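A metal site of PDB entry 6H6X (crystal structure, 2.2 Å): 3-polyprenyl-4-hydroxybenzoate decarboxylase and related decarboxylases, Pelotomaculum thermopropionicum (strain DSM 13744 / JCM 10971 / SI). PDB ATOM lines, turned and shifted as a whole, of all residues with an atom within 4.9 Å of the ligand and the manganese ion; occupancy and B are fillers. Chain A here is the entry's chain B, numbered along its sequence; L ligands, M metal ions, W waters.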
ATOM      1  N   THR A 132      -2.256 -25.756   1.473  1.00  0.00           N
ATOM      2  CA  THR A 132      -3.450 -25.570   2.282  1.00  0.00           C
ATOM      3  C   THR A 132      -4.203 -26.826   2.614  1.00  0.00           C
ATOM      4  O   THR A 132      -5.150 -26.758   3.400  1.00  0.00           O
ATOM      5  CB  THR A 132      -4.438 -24.641   1.574  1.00  0.00           C
ATOM      6  OG1 THR A 132      -4.717 -25.162   0.264  1.00  0.00           O
ATOM      7  CG2 THR A 132      -3.863 -23.241   1.449  1.00  0.00           C
ATOM      8  N   ASN A 147      -0.717 -36.517  17.196  1.00  0.00           N
ATOM      9  CA  ASN A 147      -1.753 -35.528  16.815  1.00  0.00           C
ATOM     10  C   ASN A 147      -1.713 -35.267  15.312  1.00  0.00           C
ATOM     11  O   ASN A 147      -0.661 -35.361  14.670  1.00  0.00           O
ATOM     12  CB  ASN A 147      -1.461 -34.242  17.555  1.00  0.00           C
ATOM     13  CG  ASN A 147      -2.637 -33.337  17.620  1.00  0.00           C
ATOM     14  OD1 ASN A 147      -3.547 -33.572  18.441  1.00  0.00           O
ATOM     15  ND2 ASN A 147      -2.639 -32.244  16.771  1.00  0.00           N
ATOM     16  N   VAL A 148      -2.863 -34.910  14.772  1.00  0.00           N
ATOM     17  CA  VAL A 148      -3.012 -34.480  13.400  1.00  0.00           C
ATOM     18  C   VAL A 148      -3.773 -33.143  13.411  1.00  0.00           C
ATOM     19  O   VAL A 148      -4.757 -33.007  14.103  1.00  0.00           O
ATOM     20  CB  VAL A 148      -3.809 -35.497  12.594  1.00  0.00           C
ATOM     21  CG1 VAL A 148      -3.800 -35.164  11.116  1.00  0.00           C
ATOM     22  CG2 VAL A 148      -3.211 -36.887  12.804  1.00  0.00           C
ATOM     23  N   SER A 149      -3.335 -32.191  12.594  1.00  0.00           N
ATOM     24  CA  SER A 149      -3.994 -30.908  12.359  1.00  0.00           C
ATOM     25  C   SER A 149      -3.601 -30.366  10.978  1.00  0.00           C
ATOM     26  O   SER A 149      -2.663 -30.857  10.337  1.00  0.00           O
ATOM     27  CB  SER A 149      -3.599 -29.895  13.458  1.00  0.00           C
ATOM     28  OG  SER A 149      -2.208 -29.971  13.775  1.00  0.00           O
ATOM     29  N   ILE A 150      -4.316 -29.362  10.504  1.00  0.00           N
ATOM     30  CA  ILE A 150      -4.024 -28.748   9.213  1.00  0.00           C
ATOM     31  C   ILE A 150      -3.564 -27.315   9.484  1.00  0.00           C
ATOM     32  O   ILE A 150      -4.274 -26.542  10.160  1.00  0.00           O
ATOM     33  CB  ILE A 150      -5.259 -28.744   8.288  1.00  0.00           C
ATOM     34  CG1 ILE A 150      -5.609 -30.186   7.916  1.00  0.00           C
ATOM     35  CG2 ILE A 150      -4.989 -27.922   7.032  1.00  0.00           C
ATOM     36  CD1 ILE A 150      -6.798 -30.314   6.958  1.00  0.00           C
ATOM     37  N   HIS A 151      -2.413 -26.979   8.917  1.00  0.00           N
ATOM     38  CA  HIS A 151      -1.795 -25.634   9.047  1.00  0.00           C
ATOM     39  C   HIS A 151      -1.424 -25.121   7.668  1.00  0.00           C
ATOM     40  O   HIS A 151      -0.996 -25.893   6.802  1.00  0.00           O
ATOM     41  CB  HIS A 151      -0.519 -25.717   9.913  1.00  0.00           C
ATOM     42  CG  HIS A 151      -0.784 -26.289  11.261  1.00  0.00           C
ATOM     43  ND1 HIS A 151      -1.086 -25.507  12.360  1.00  0.00           N
ATOM     44  CD2 HIS A 151      -0.969 -27.585  11.661  1.00  0.00           C
ATOM     45  CE1 HIS A 151      -1.399 -26.297  13.380  1.00  0.00           C
ATOM     46  NE2 HIS A 151      -1.319 -27.557  12.978  1.00  0.00           N
ATOM     47  N   ARG A 152      -1.658 -23.833   7.434  1.00  0.00           N
ATOM     48  CA  ARG A 152      -1.165 -23.230   6.196  1.00  0.00           C
ATOM     49  C   ARG A 152       0.354 -23.191   6.209  1.00  0.00           C
ATOM     50  O   ARG A 152       0.962 -22.969   7.247  1.00  0.00           O
ATOM     51  CB  ARG A 152      -1.790 -21.847   5.976  1.00  0.00           C
ATOM     52  CG  ARG A 152      -1.227 -20.780   6.870  1.00  0.00           C
ATOM     53  CD  ARG A 152      -1.966 -19.470   6.725  1.00  0.00           C
ATOM     54  NE  ARG A 152      -1.253 -18.384   7.403  1.00  0.00           N
ATOM     55  CZ  ARG A 152      -1.796 -17.337   8.041  1.00  0.00           C
ATOM     56  NH1 ARG A 152      -3.093 -17.162   8.163  1.00  0.00           N
ATOM     57  NH2 ARG A 152      -0.983 -16.463   8.599  1.00  0.00           N
ATOM     58  N   LEU A 164       1.875 -21.234  10.282  1.00  0.00           N
ATOM     59  CA  LEU A 164       1.053 -20.655  11.301  1.00  0.00           C
ATOM     60  C   LEU A 164       0.626 -21.768  12.241  1.00  0.00           C
ATOM     61  O   LEU A 164      -0.057 -22.704  11.808  1.00  0.00           O
ATOM     62  CB  LEU A 164      -0.186 -19.993  10.674  1.00  0.00           C
ATOM     63  CG  LEU A 164      -1.268 -19.608  11.738  1.00  0.00           C
ATOM     64  CD1 LEU A 164      -0.710 -18.554  12.701  1.00  0.00           C
ATOM     65  CD2 LEU A 164      -2.534 -19.138  11.060  1.00  0.00           C
ATOM     66  N   ILE A 165       1.037 -21.701  13.508  1.00  0.00           N
ATOM     67  CA  ILE A 165       0.571 -22.617  14.532  1.00  0.00           C
ATOM     68  C   ILE A 165      -0.234 -21.835  15.611  1.00  0.00           C
ATOM     69  O   ILE A 165       0.313 -21.118  16.425  1.00  0.00           O
ATOM     70  CB  ILE A 165       1.738 -23.379  15.190  1.00  0.00           C
ATOM     71  CG1 ILE A 165       2.721 -23.924  14.132  1.00  0.00           C
ATOM     72  CG2 ILE A 165       1.250 -24.550  16.018  1.00  0.00           C
ATOM     73  CD1 ILE A 165       3.893 -24.661  14.764  1.00  0.00           C
ATOM     74  N   LEU A 166      -1.542 -22.023  15.628  1.00  0.00           N
ATOM     75  CA  LEU A 166      -2.393 -21.509  16.695  1.00  0.00           C
ATOM     76  C   LEU A 166      -2.155 -22.256  18.009  1.00  0.00           C
ATOM     77  O   LEU A 166      -1.633 -23.366  17.996  1.00  0.00           O
ATOM     78  CB  LEU A 166      -3.853 -21.537  16.246  1.00  0.00           C
ATOM     79  CG  LEU A 166      -4.116 -20.596  15.036  1.00  0.00           C
ATOM     80  CD1 LEU A 166      -5.537 -20.708  14.475  1.00  0.00           C
ATOM     81  CD2 LEU A 166      -3.820 -19.120  15.405  1.00  0.00           C
ATOM     82  N   ARG A 168      -2.840 -24.570  20.239  1.00  0.00           N
ATOM     83  CA  ARG A 168      -3.649 -25.793  20.363  1.00  0.00           C
ATOM     84  C   ARG A 168      -2.647 -26.964  20.513  1.00  0.00           C
ATOM     85  O   ARG A 168      -1.581 -26.755  21.101  1.00  0.00           O
ATOM     86  CB  ARG A 168      -4.580 -25.953  19.139  1.00  0.00           C
ATOM     87  CG  ARG A 168      -5.724 -24.939  18.954  1.00  0.00           C
ATOM     88  CD  ARG A 168      -6.946 -25.252  19.844  1.00  0.00           C
ATOM     89  NE  ARG A 168      -7.368 -26.674  19.820  1.00  0.00           N
ATOM     90  CZ  ARG A 168      -7.742 -27.426  20.858  1.00  0.00           C
ATOM     91  NH1 ARG A 168      -7.802 -26.937  22.092  1.00  0.00           N
ATOM     92  NH2 ARG A 168      -8.069 -28.700  20.666  1.00  0.00           N
ATOM     93  N   HIS A 169      -2.899 -28.176  19.976  1.00  0.00           N
ATOM     94  CA  HIS A 169      -2.008 -29.290  20.291  1.00  0.00           C
ATOM     95  C   HIS A 169      -0.598 -29.241  19.708  1.00  0.00           C
ATOM     96  O   HIS A 169       0.365 -29.513  20.394  1.00  0.00           O
ATOM     97  CB  HIS A 169      -2.679 -30.635  20.008  1.00  0.00           C
ATOM     98  CG  HIS A 169      -3.909 -30.842  20.825  1.00  0.00           C
ATOM     99  ND1 HIS A 169      -4.912 -31.717  20.459  1.00  0.00           N
ATOM    100  CD2 HIS A 169      -4.334 -30.245  21.969  1.00  0.00           C
ATOM    101  CE1 HIS A 169      -5.882 -31.672  21.361  1.00  0.00           C
ATOM    102  NE2 HIS A 169      -5.560 -30.783  22.282  1.00  0.00           N
ATOM    103  N   LEU A 170      -0.460 -28.902  18.426  1.00  0.00           N
ATOM    104  CA  LEU A 170       0.860 -28.860  17.854  1.00  0.00           C
ATOM    105  C   LEU A 170       1.765 -27.825  18.577  1.00  0.00           C
ATOM    106  O   LEU A 170       2.930 -28.050  18.775  1.00  0.00           O
ATOM    107  CB  LEU A 170       0.751 -28.501  16.387  1.00  0.00           C
ATOM    108  CG  LEU A 170       2.081 -28.483  15.661  1.00  0.00           C
ATOM    109  CD1 LEU A 170       2.736 -29.823  15.725  1.00  0.00           C
ATOM    110  CD2 LEU A 170       1.833 -28.061  14.241  1.00  0.00           C
ATOM    111  N   SER A 200      -8.981 -34.845  10.951  1.00  0.00           N
ATOM    112  CA  SER A 200      -7.926 -33.913  11.396  1.00  0.00           C
ATOM    113  C   SER A 200      -8.450 -32.654  12.075  1.00  0.00           C
ATOM    114  O   SER A 200      -7.673 -31.924  12.715  1.00  0.00           O
ATOM    115  CB  SER A 200      -7.059 -33.497  10.231  1.00  0.00           C
ATOM    116  OG  SER A 200      -7.765 -32.578   9.394  1.00  0.00           O
ATOM    117  N   GLN A 201      -9.740 -32.367  11.894  1.00  0.00           N
ATOM    118  CA  GLN A 201     -10.401 -31.215  12.492  1.00  0.00           C
ATOM    119  C   GLN A 201     -11.102 -31.512  13.826  1.00  0.00           C
ATOM    120  O   GLN A 201     -11.615 -30.587  14.423  1.00  0.00           O
ATOM    121  CB  GLN A 201     -11.391 -30.624  11.465  1.00  0.00           C
ATOM    122  CG  GLN A 201     -10.691 -30.203  10.193  1.00  0.00           C
ATOM    123  CD  GLN A 201      -9.573 -29.205  10.501  1.00  0.00           C
ATOM    124  OE1 GLN A 201      -8.372 -29.519  10.432  1.00  0.00           O
ATOM    125  NE2 GLN A 201      -9.963 -28.019  10.924  1.00  0.00           N
ATOM    126  N   ALA A 202     -11.092 -32.742  14.297  1.00  0.00           N
ATOM    127  CA  ALA A 202     -11.570 -33.019  15.657  1.00  0.00           C
ATOM    128  C   ALA A 202     -10.794 -32.237  16.732  1.00  0.00           C
ATOM    129  O   ALA A 202      -9.544 -32.176  16.761  1.00  0.00           O
ATOM    130  CB  ALA A 202     -11.517 -34.508  15.979  1.00  0.00           C
ATOM    131  N   THR A 203     -11.587 -31.631  17.602  1.00  0.00           N
ATOM    132  CA  THR A 203     -11.146 -30.936  18.777  1.00  0.00           C
ATOM    133  C   THR A 203     -11.417 -31.921  19.894  1.00  0.00           C
ATOM    134  O   THR A 203     -12.562 -32.310  20.170  1.00  0.00           O
ATOM    135  CB  THR A 203     -11.949 -29.625  18.966  1.00  0.00           C
ATOM    136  OG1 THR A 203     -11.814 -28.844  17.765  1.00  0.00           O
ATOM    137  CG2 THR A 203     -11.446 -28.792  20.177  1.00  0.00           C
ATOM    138  N   THR A 204     -10.336 -32.358  20.513  1.00  0.00           N
ATOM    139  CA  THR A 204     -10.392 -33.341  21.569  1.00  0.00           C
ATOM    140  C   THR A 204      -9.534 -32.882  22.745  1.00  0.00           C
ATOM    141  O   THR A 204      -8.802 -31.871  22.639  1.00  0.00           O
ATOM    142  CB  THR A 204      -9.861 -34.709  21.092  1.00  0.00           C
ATOM    143  OG1 THR A 204      -8.437 -34.717  21.124  1.00  0.00           O
ATOM    144  CG2 THR A 204     -10.317 -35.039  19.636  1.00  0.00           C
ATOM    145  N   VAL A 208      -5.718 -37.732  22.188  1.00  0.00           N
ATOM    146  CA  VAL A 208      -6.388 -38.692  21.287  1.00  0.00           C
ATOM    147  C   VAL A 208      -5.954 -38.439  19.850  1.00  0.00           C
ATOM    148  O   VAL A 208      -5.946 -37.313  19.335  1.00  0.00           O
ATOM    149  CB  VAL A 208      -7.927 -38.810  21.464  1.00  0.00           C
ATOM    150  CG1 VAL A 208      -8.588 -37.487  21.391  1.00  0.00           C
ATOM    151  CG2 VAL A 208      -8.550 -39.693  20.419  1.00  0.00           C
ATOM    152  N   GLU A 210      -5.889 -38.293  16.161  1.00  0.00           N
ATOM    153  CA  GLU A 210      -6.860 -38.126  15.094  1.00  0.00           C
ATOM    154  C   GLU A 210      -6.725 -39.156  13.965  1.00  0.00           C
ATOM    155  O   GLU A 210      -7.708 -39.396  13.249  1.00  0.00           O
ATOM    156  CB  GLU A 210      -6.859 -36.731  14.542  1.00  0.00           C
ATOM    157  CG  GLU A 210      -7.376 -35.745  15.561  1.00  0.00           C
ATOM    158  CD  GLU A 210      -6.248 -35.076  16.385  1.00  0.00           C
ATOM    159  OE1 GLU A 210      -5.150 -35.601  16.495  1.00  0.00           O
ATOM    160  OE2 GLU A 210      -6.480 -33.991  16.878  1.00  0.00           O
ATOM    161  N   PHE A 257      -1.990 -13.737   4.542  1.00  0.00           N
ATOM    162  CA  PHE A 257      -2.732 -14.801   3.825  1.00  0.00           C
ATOM    163  C   PHE A 257      -4.233 -14.556   3.898  1.00  0.00           C
ATOM    164  O   PHE A 257      -4.760 -14.271   4.976  1.00  0.00           O
ATOM    165  CB  PHE A 257      -2.339 -16.119   4.506  1.00  0.00           C
ATOM    166  CG  PHE A 257      -2.979 -17.353   3.950  1.00  0.00           C
ATOM    167  CD1 PHE A 257      -2.556 -17.921   2.800  1.00  0.00           C
ATOM    168  CD2 PHE A 257      -4.015 -17.965   4.643  1.00  0.00           C
ATOM    169  CE1 PHE A 257      -3.131 -19.086   2.312  1.00  0.00           C
ATOM    170  CE2 PHE A 257      -4.587 -19.161   4.186  1.00  0.00           C
ATOM    171  CZ  PHE A 257      -4.103 -19.732   3.041  1.00  0.00           C
ATOM    172  N   GLU A 259      -7.811 -15.699   4.658  1.00  0.00           N
ATOM    173  CA  GLU A 259      -8.257 -16.738   5.607  1.00  0.00           C
ATOM    174  C   GLU A 259      -9.787 -17.018   5.576  1.00  0.00           C
ATOM    175  O   GLU A 259     -10.508 -16.365   4.850  1.00  0.00           O
ATOM    176  CB  GLU A 259      -7.808 -16.326   7.031  1.00  0.00           C
ATOM    177  CG  GLU A 259      -6.547 -17.004   7.567  1.00  0.00           C
ATOM    178  CD  GLU A 259      -6.629 -18.541   7.727  1.00  0.00           C
ATOM    179  OE1 GLU A 259      -5.634 -19.077   8.279  1.00  0.00           O
ATOM    180  OE2 GLU A 259      -7.638 -19.244   7.320  1.00  0.00           O
ATOM    181  N   ILE A 289      -6.999 -26.720  -1.012  1.00  0.00           N
ATOM    182  CA  ILE A 289      -8.249 -26.228  -0.481  1.00  0.00           C
ATOM    183  C   ILE A 289      -8.221 -24.731  -0.640  1.00  0.00           C
ATOM    184  O   ILE A 289      -7.281 -24.083  -0.198  1.00  0.00           O
ATOM    185  CB  ILE A 289      -8.414 -26.641   0.988  1.00  0.00           C
ATOM    186  CG1 ILE A 289      -8.762 -28.121   1.100  1.00  0.00           C
ATOM    187  CG2 ILE A 289      -9.473 -25.778   1.719  1.00  0.00           C
ATOM    188  CD1 ILE A 289      -8.495 -28.656   2.512  1.00  0.00           C
ATOM    189  N   PRO A 291      -9.049 -21.137   0.339  1.00  0.00           N
ATOM    190  CA  PRO A 291      -9.542 -20.654   1.641  1.00  0.00           C
ATOM    191  C   PRO A 291     -10.871 -19.947   1.560  1.00  0.00           C
ATOM    192  O   PRO A 291     -11.150 -19.287   0.570  1.00  0.00           O
ATOM    193  CB  PRO A 291      -8.445 -19.686   2.077  1.00  0.00           C
ATOM    194  CG  PRO A 291      -7.243 -20.290   1.540  1.00  0.00           C
ATOM    195  CD  PRO A 291      -7.654 -20.730   0.159  1.00  0.00           C
ATOM    196  N   HIS A 296     -13.467 -25.626   2.687  1.00  0.00           N
ATOM    197  CA  HIS A 296     -12.752 -25.153   3.852  1.00  0.00           C
ATOM    198  C   HIS A 296     -13.693 -25.012   5.033  1.00  0.00           C
ATOM    199  O   HIS A 296     -13.433 -25.549   6.096  1.00  0.00           O
ATOM    200  CB  HIS A 296     -12.044 -23.853   3.538  1.00  0.00           C
ATOM    201  CG  HIS A 296     -11.254 -23.309   4.677  1.00  0.00           C
ATOM    202  ND1 HIS A 296     -10.849 -21.992   4.722  1.00  0.00           N
ATOM    203  CD2 HIS A 296     -10.790 -23.888   5.825  1.00  0.00           C
ATOM    204  CE1 HIS A 296     -10.175 -21.775   5.831  1.00  0.00           C
ATOM    205  NE2 HIS A 296     -10.136 -22.905   6.530  1.00  0.00           N
ATOM    206  N   LEU A 299     -15.258 -28.482   6.354  1.00  0.00           N
ATOM    207  CA  LEU A 299     -14.322 -29.410   7.012  1.00  0.00           C
ATOM    208  C   LEU A 299     -14.264 -29.093   8.482  1.00  0.00           C
ATOM    209  O   LEU A 299     -14.487 -29.974   9.284  1.00  0.00           O
ATOM    210  CB  LEU A 299     -12.882 -29.346   6.468  1.00  0.00           C
ATOM    211  CG  LEU A 299     -12.476 -30.320   5.398  1.00  0.00           C
ATOM    212  CD1 LEU A 299     -11.071 -30.010   4.917  1.00  0.00           C
ATOM    213  CD2 LEU A 299     -12.540 -31.729   5.952  1.00  0.00           C
ATOM    214  N   GLY A 300     -13.940 -27.866   8.821  1.00  0.00           N
ATOM    215  CA  GLY A 300     -13.921 -27.413  10.190  1.00  0.00           C
ATOM    216  C   GLY A 300     -15.292 -27.351  10.847  1.00  0.00           C
ATOM    217  O   GLY A 300     -15.450 -27.777  11.999  1.00  0.00           O
HETATM  218  C1  LIG L   1      -7.959 -25.970   9.258  1.00  0.00           C
HETATM  219  C2  LIG L   1      -8.305 -26.203   7.898  1.00  0.00           C
HETATM  220  C3  LIG L   1      -7.701 -25.500   6.833  1.00  0.00           C
HETATM  221  C4  LIG L   1      -5.465 -23.944  11.184  1.00  0.00           C
HETATM  222  C5  LIG L   1      -6.885 -24.304   7.149  1.00  0.00           C
HETATM  223  N1  LIG L   1      -2.928 -22.869  11.673  1.00  0.00           N
HETATM  224  C6  LIG L   1      -3.613 -23.518  12.658  1.00  0.00           C
HETATM  225  C7  LIG L   1      -6.486 -23.191   4.615  1.00  0.00           C
HETATM  226  C8  LIG L   1      -6.197 -23.394   6.093  1.00  0.00           C
HETATM  227  C9  LIG L   1      -5.420 -21.998   8.040  1.00  0.00           C
HETATM  228  O1  LIG L   1      -3.071 -23.608  13.794  1.00  0.00           O
HETATM  229  N2  LIG L   1      -4.857 -24.047  12.402  1.00  0.00           N
HETATM  230  C10 LIG L   1      -3.432 -22.729  10.427  1.00  0.00           C
HETATM  231  O2  LIG L   1      -2.735 -22.188   9.558  1.00  0.00           O
HETATM  232  C11 LIG L   1      -4.789 -23.315  10.136  1.00  0.00           C
HETATM  233  N3  LIG L   1      -5.401 -23.268   8.848  1.00  0.00           N
HETATM  234  C12 LIG L   1      -5.667 -22.149   6.725  1.00  0.00           C
HETATM  235  C13 LIG L   1      -4.875 -24.214   5.805  1.00  0.00           C
HETATM  236  C14 LIG L   1      -6.412 -24.201   8.523  1.00  0.00           C
HETATM  237  C15 LIG L   1      -8.073 -25.739   5.415  1.00  0.00           C
HETATM  238  C16 LIG L   1      -9.271 -27.343   7.669  1.00  0.00           C
HETATM  239  C17 LIG L   1      -7.058 -24.964   9.614  1.00  0.00           C
HETATM  240  N4  LIG L   1      -6.743 -24.537  10.935  1.00  0.00           N
HETATM  241  C18 LIG L   1      -7.409 -25.176  12.076  1.00  0.00           C
HETATM  242  C19 LIG L   1      -6.816 -26.521  12.588  1.00  0.00           C
HETATM  243  O3  LIG L   1      -6.373 -27.485  11.561  1.00  0.00           O
HETATM  244  C20 LIG L   1      -7.920 -27.139  13.484  1.00  0.00           C
HETATM  245  O4  LIG L   1      -8.452 -26.255  14.499  1.00  0.00           O
HETATM  246  C21 LIG L   1      -7.341 -28.360  14.189  1.00  0.00           C
HETATM  247  O5  LIG L   1      -8.428 -29.175  14.657  1.00  0.00           O
HETATM  248  C22 LIG L   1      -6.448 -28.048  15.408  1.00  0.00           C
HETATM  249  O6  LIG L   1      -6.086 -29.369  15.864  1.00  0.00           O
HETATM  250  P1  LIG L   1      -5.655 -29.729  17.370  1.00  0.00           P
HETATM  251  O7  LIG L   1      -5.102 -31.105  17.249  1.00  0.00           O
HETATM  252  O8  LIG L   1      -4.587 -28.710  17.801  1.00  0.00           O
HETATM  253  O9  LIG L   1      -6.922 -29.622  18.217  1.00  0.00           O
HETATM  254 MN    MN M   1      -5.443 -32.873  18.585  1.00  0.00          MN
HETATM  255  O   HOH W   1      -5.735 -34.886  19.805  1.00  0.00           O
HETATM  256  O   HOH W   2      -9.493 -22.461   9.804  1.00  0.00           O
HETATM  257  O   HOH W   3      -9.266 -28.376  17.215  1.00  0.00           O
HETATM  258  O   HOH W   4      -7.659 -32.034  18.743  1.00  0.00           O
HETATM  259  O   HOH W   5     -10.061 -24.004  14.280  1.00  0.00           O
HETATM  260  O   HOH W   6      -2.637 -28.355  16.419  1.00  0.00           O
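The backbone carbonyl oxygen of Ser 200 lies within hydrogen-bond range of an oxygen (O5) of the ligand (3.4 Å).
The backbone NH (N) of Ile 150 sits at hydrogen-bond distance from an oxygen (O3) of the ligand (3.0 Å).
ND1 of His 151 is in hydrogen-bond range of O1 of the ligand (3.1 Å).
N1 of the ligand lies within hydrogen-bond range of O of Leu 164.
N of Leu 166 sits at hydrogen-bond distance from O1 of the ligand (2.9 Å).
OE1 of Gln 201 sits at hydrogen-bond distance from O3 of the ligand (3.1 Å).
The guanidinium group (NH2) of Arg 168 lies within salt-bridge range of an oxygen (O9) of the ligand (2.9 Å).
An oxygen (O3) of the ligand is in hydrogen-bond range of the backbone carbonyl oxygen (O) of Ile 150.
O of Gln 201 lies within hydrogen-bond range of O5 of the ligand (3.5 Å).
O8 of the ligand lies within hydrogen-bond range of N of His 169.
The backbone NH of Arg 152 is in hydrogen-bond range of an oxygen (O2) of the ligand.
NE2 of His 169 sits close to O of Thr 204, 3.4 Å away.
O of Ile 289 sits at hydrogen-bond distance from OG1 of Thr 132, 2.8 Å away.
A ring nitrogen (NE2) of His 151 is in hydrogen-bond range of the side-chain hydroxyl of Ser 149.
O of Leu 164 lies within hydrogen-bond range of ND1 of His 151 (3.0 Å).
The side-chain amide oxygen (OE1) of Gln 201 is in hydrogen-bond range of the side-chain hydroxyl (OG) of Ser 200 (3.3 Å).
NH1 of Arg 152 lies within salt-bridge range of OE1 of Glu 259 (3.2 Å).
The backbone NH (N) of Val 148 lies within hydrogen-bond range of the side-chain carboxylate (OE1) of Glu 210, 2.9 Å away.
Thr 132 touches the ligand (O to C13, 3.5 Å).
O of Val 148 touches O7 of the ligand, at 3.7 Å.
CB of Ser 149 touches O6 of the ligand (3.5 Å).
Ile 165 touches the ligand.
Ala 202 touches the ligand.
Glu 259 touches the ligand (OE1 to C9, 2.9 Å).
Ile 289 touches the ligand (CG2 to C15, 3.95 Å).
His 296 touches the ligand.
Hydrophobic or aromatic side chains within 4 Å of the ligand: Ile 150, His 151, Leu 164, Leu 166, His 169, Ile 289 and His 296.
Along chain A the residues within 4 Å of the ligand span positions 132 to 296.
The nearest printed residue that does not touch the ligand is Phe 257 (4.1 Å).
Of the 27 residues printed, 3 come within 4 Å of the manganese ion.
The manganese ion is bound by the side-chain amide oxygen of Asn 147 (2.0 Å), an oxygen (O7) of the ligand (2.2 Å), a ring nitrogen (ND1) of His 169 (2.3 Å), the side-chain carboxylate of Glu 210 (2.3 Å), water W1 (2.4 Å) and water W4 (2.4 Å).
Water W4 lies within hydrogen-bond range of O9 of the ligand (2.6 Å), O of Ala 202 (2.7 Å) and N of Thr 204 (3.2 Å).
Water W1 lies within hydrogen-bond range of O of Val 208 (2.5 Å), OG1 of Thr 204 (3.0 Å) and OE1 of Glu 210 (3.4 Å).
Water W6 lies within hydrogen-bond range of an oxygen (O8) of the ligand, the backbone NH (N) of Leu 170 and the side-chain hydroxyl (OG) of Ser 149.
Water W3 bridges OG1 of Thr 203 (2.6 Å) and O5 of the ligand (2.8 Å).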
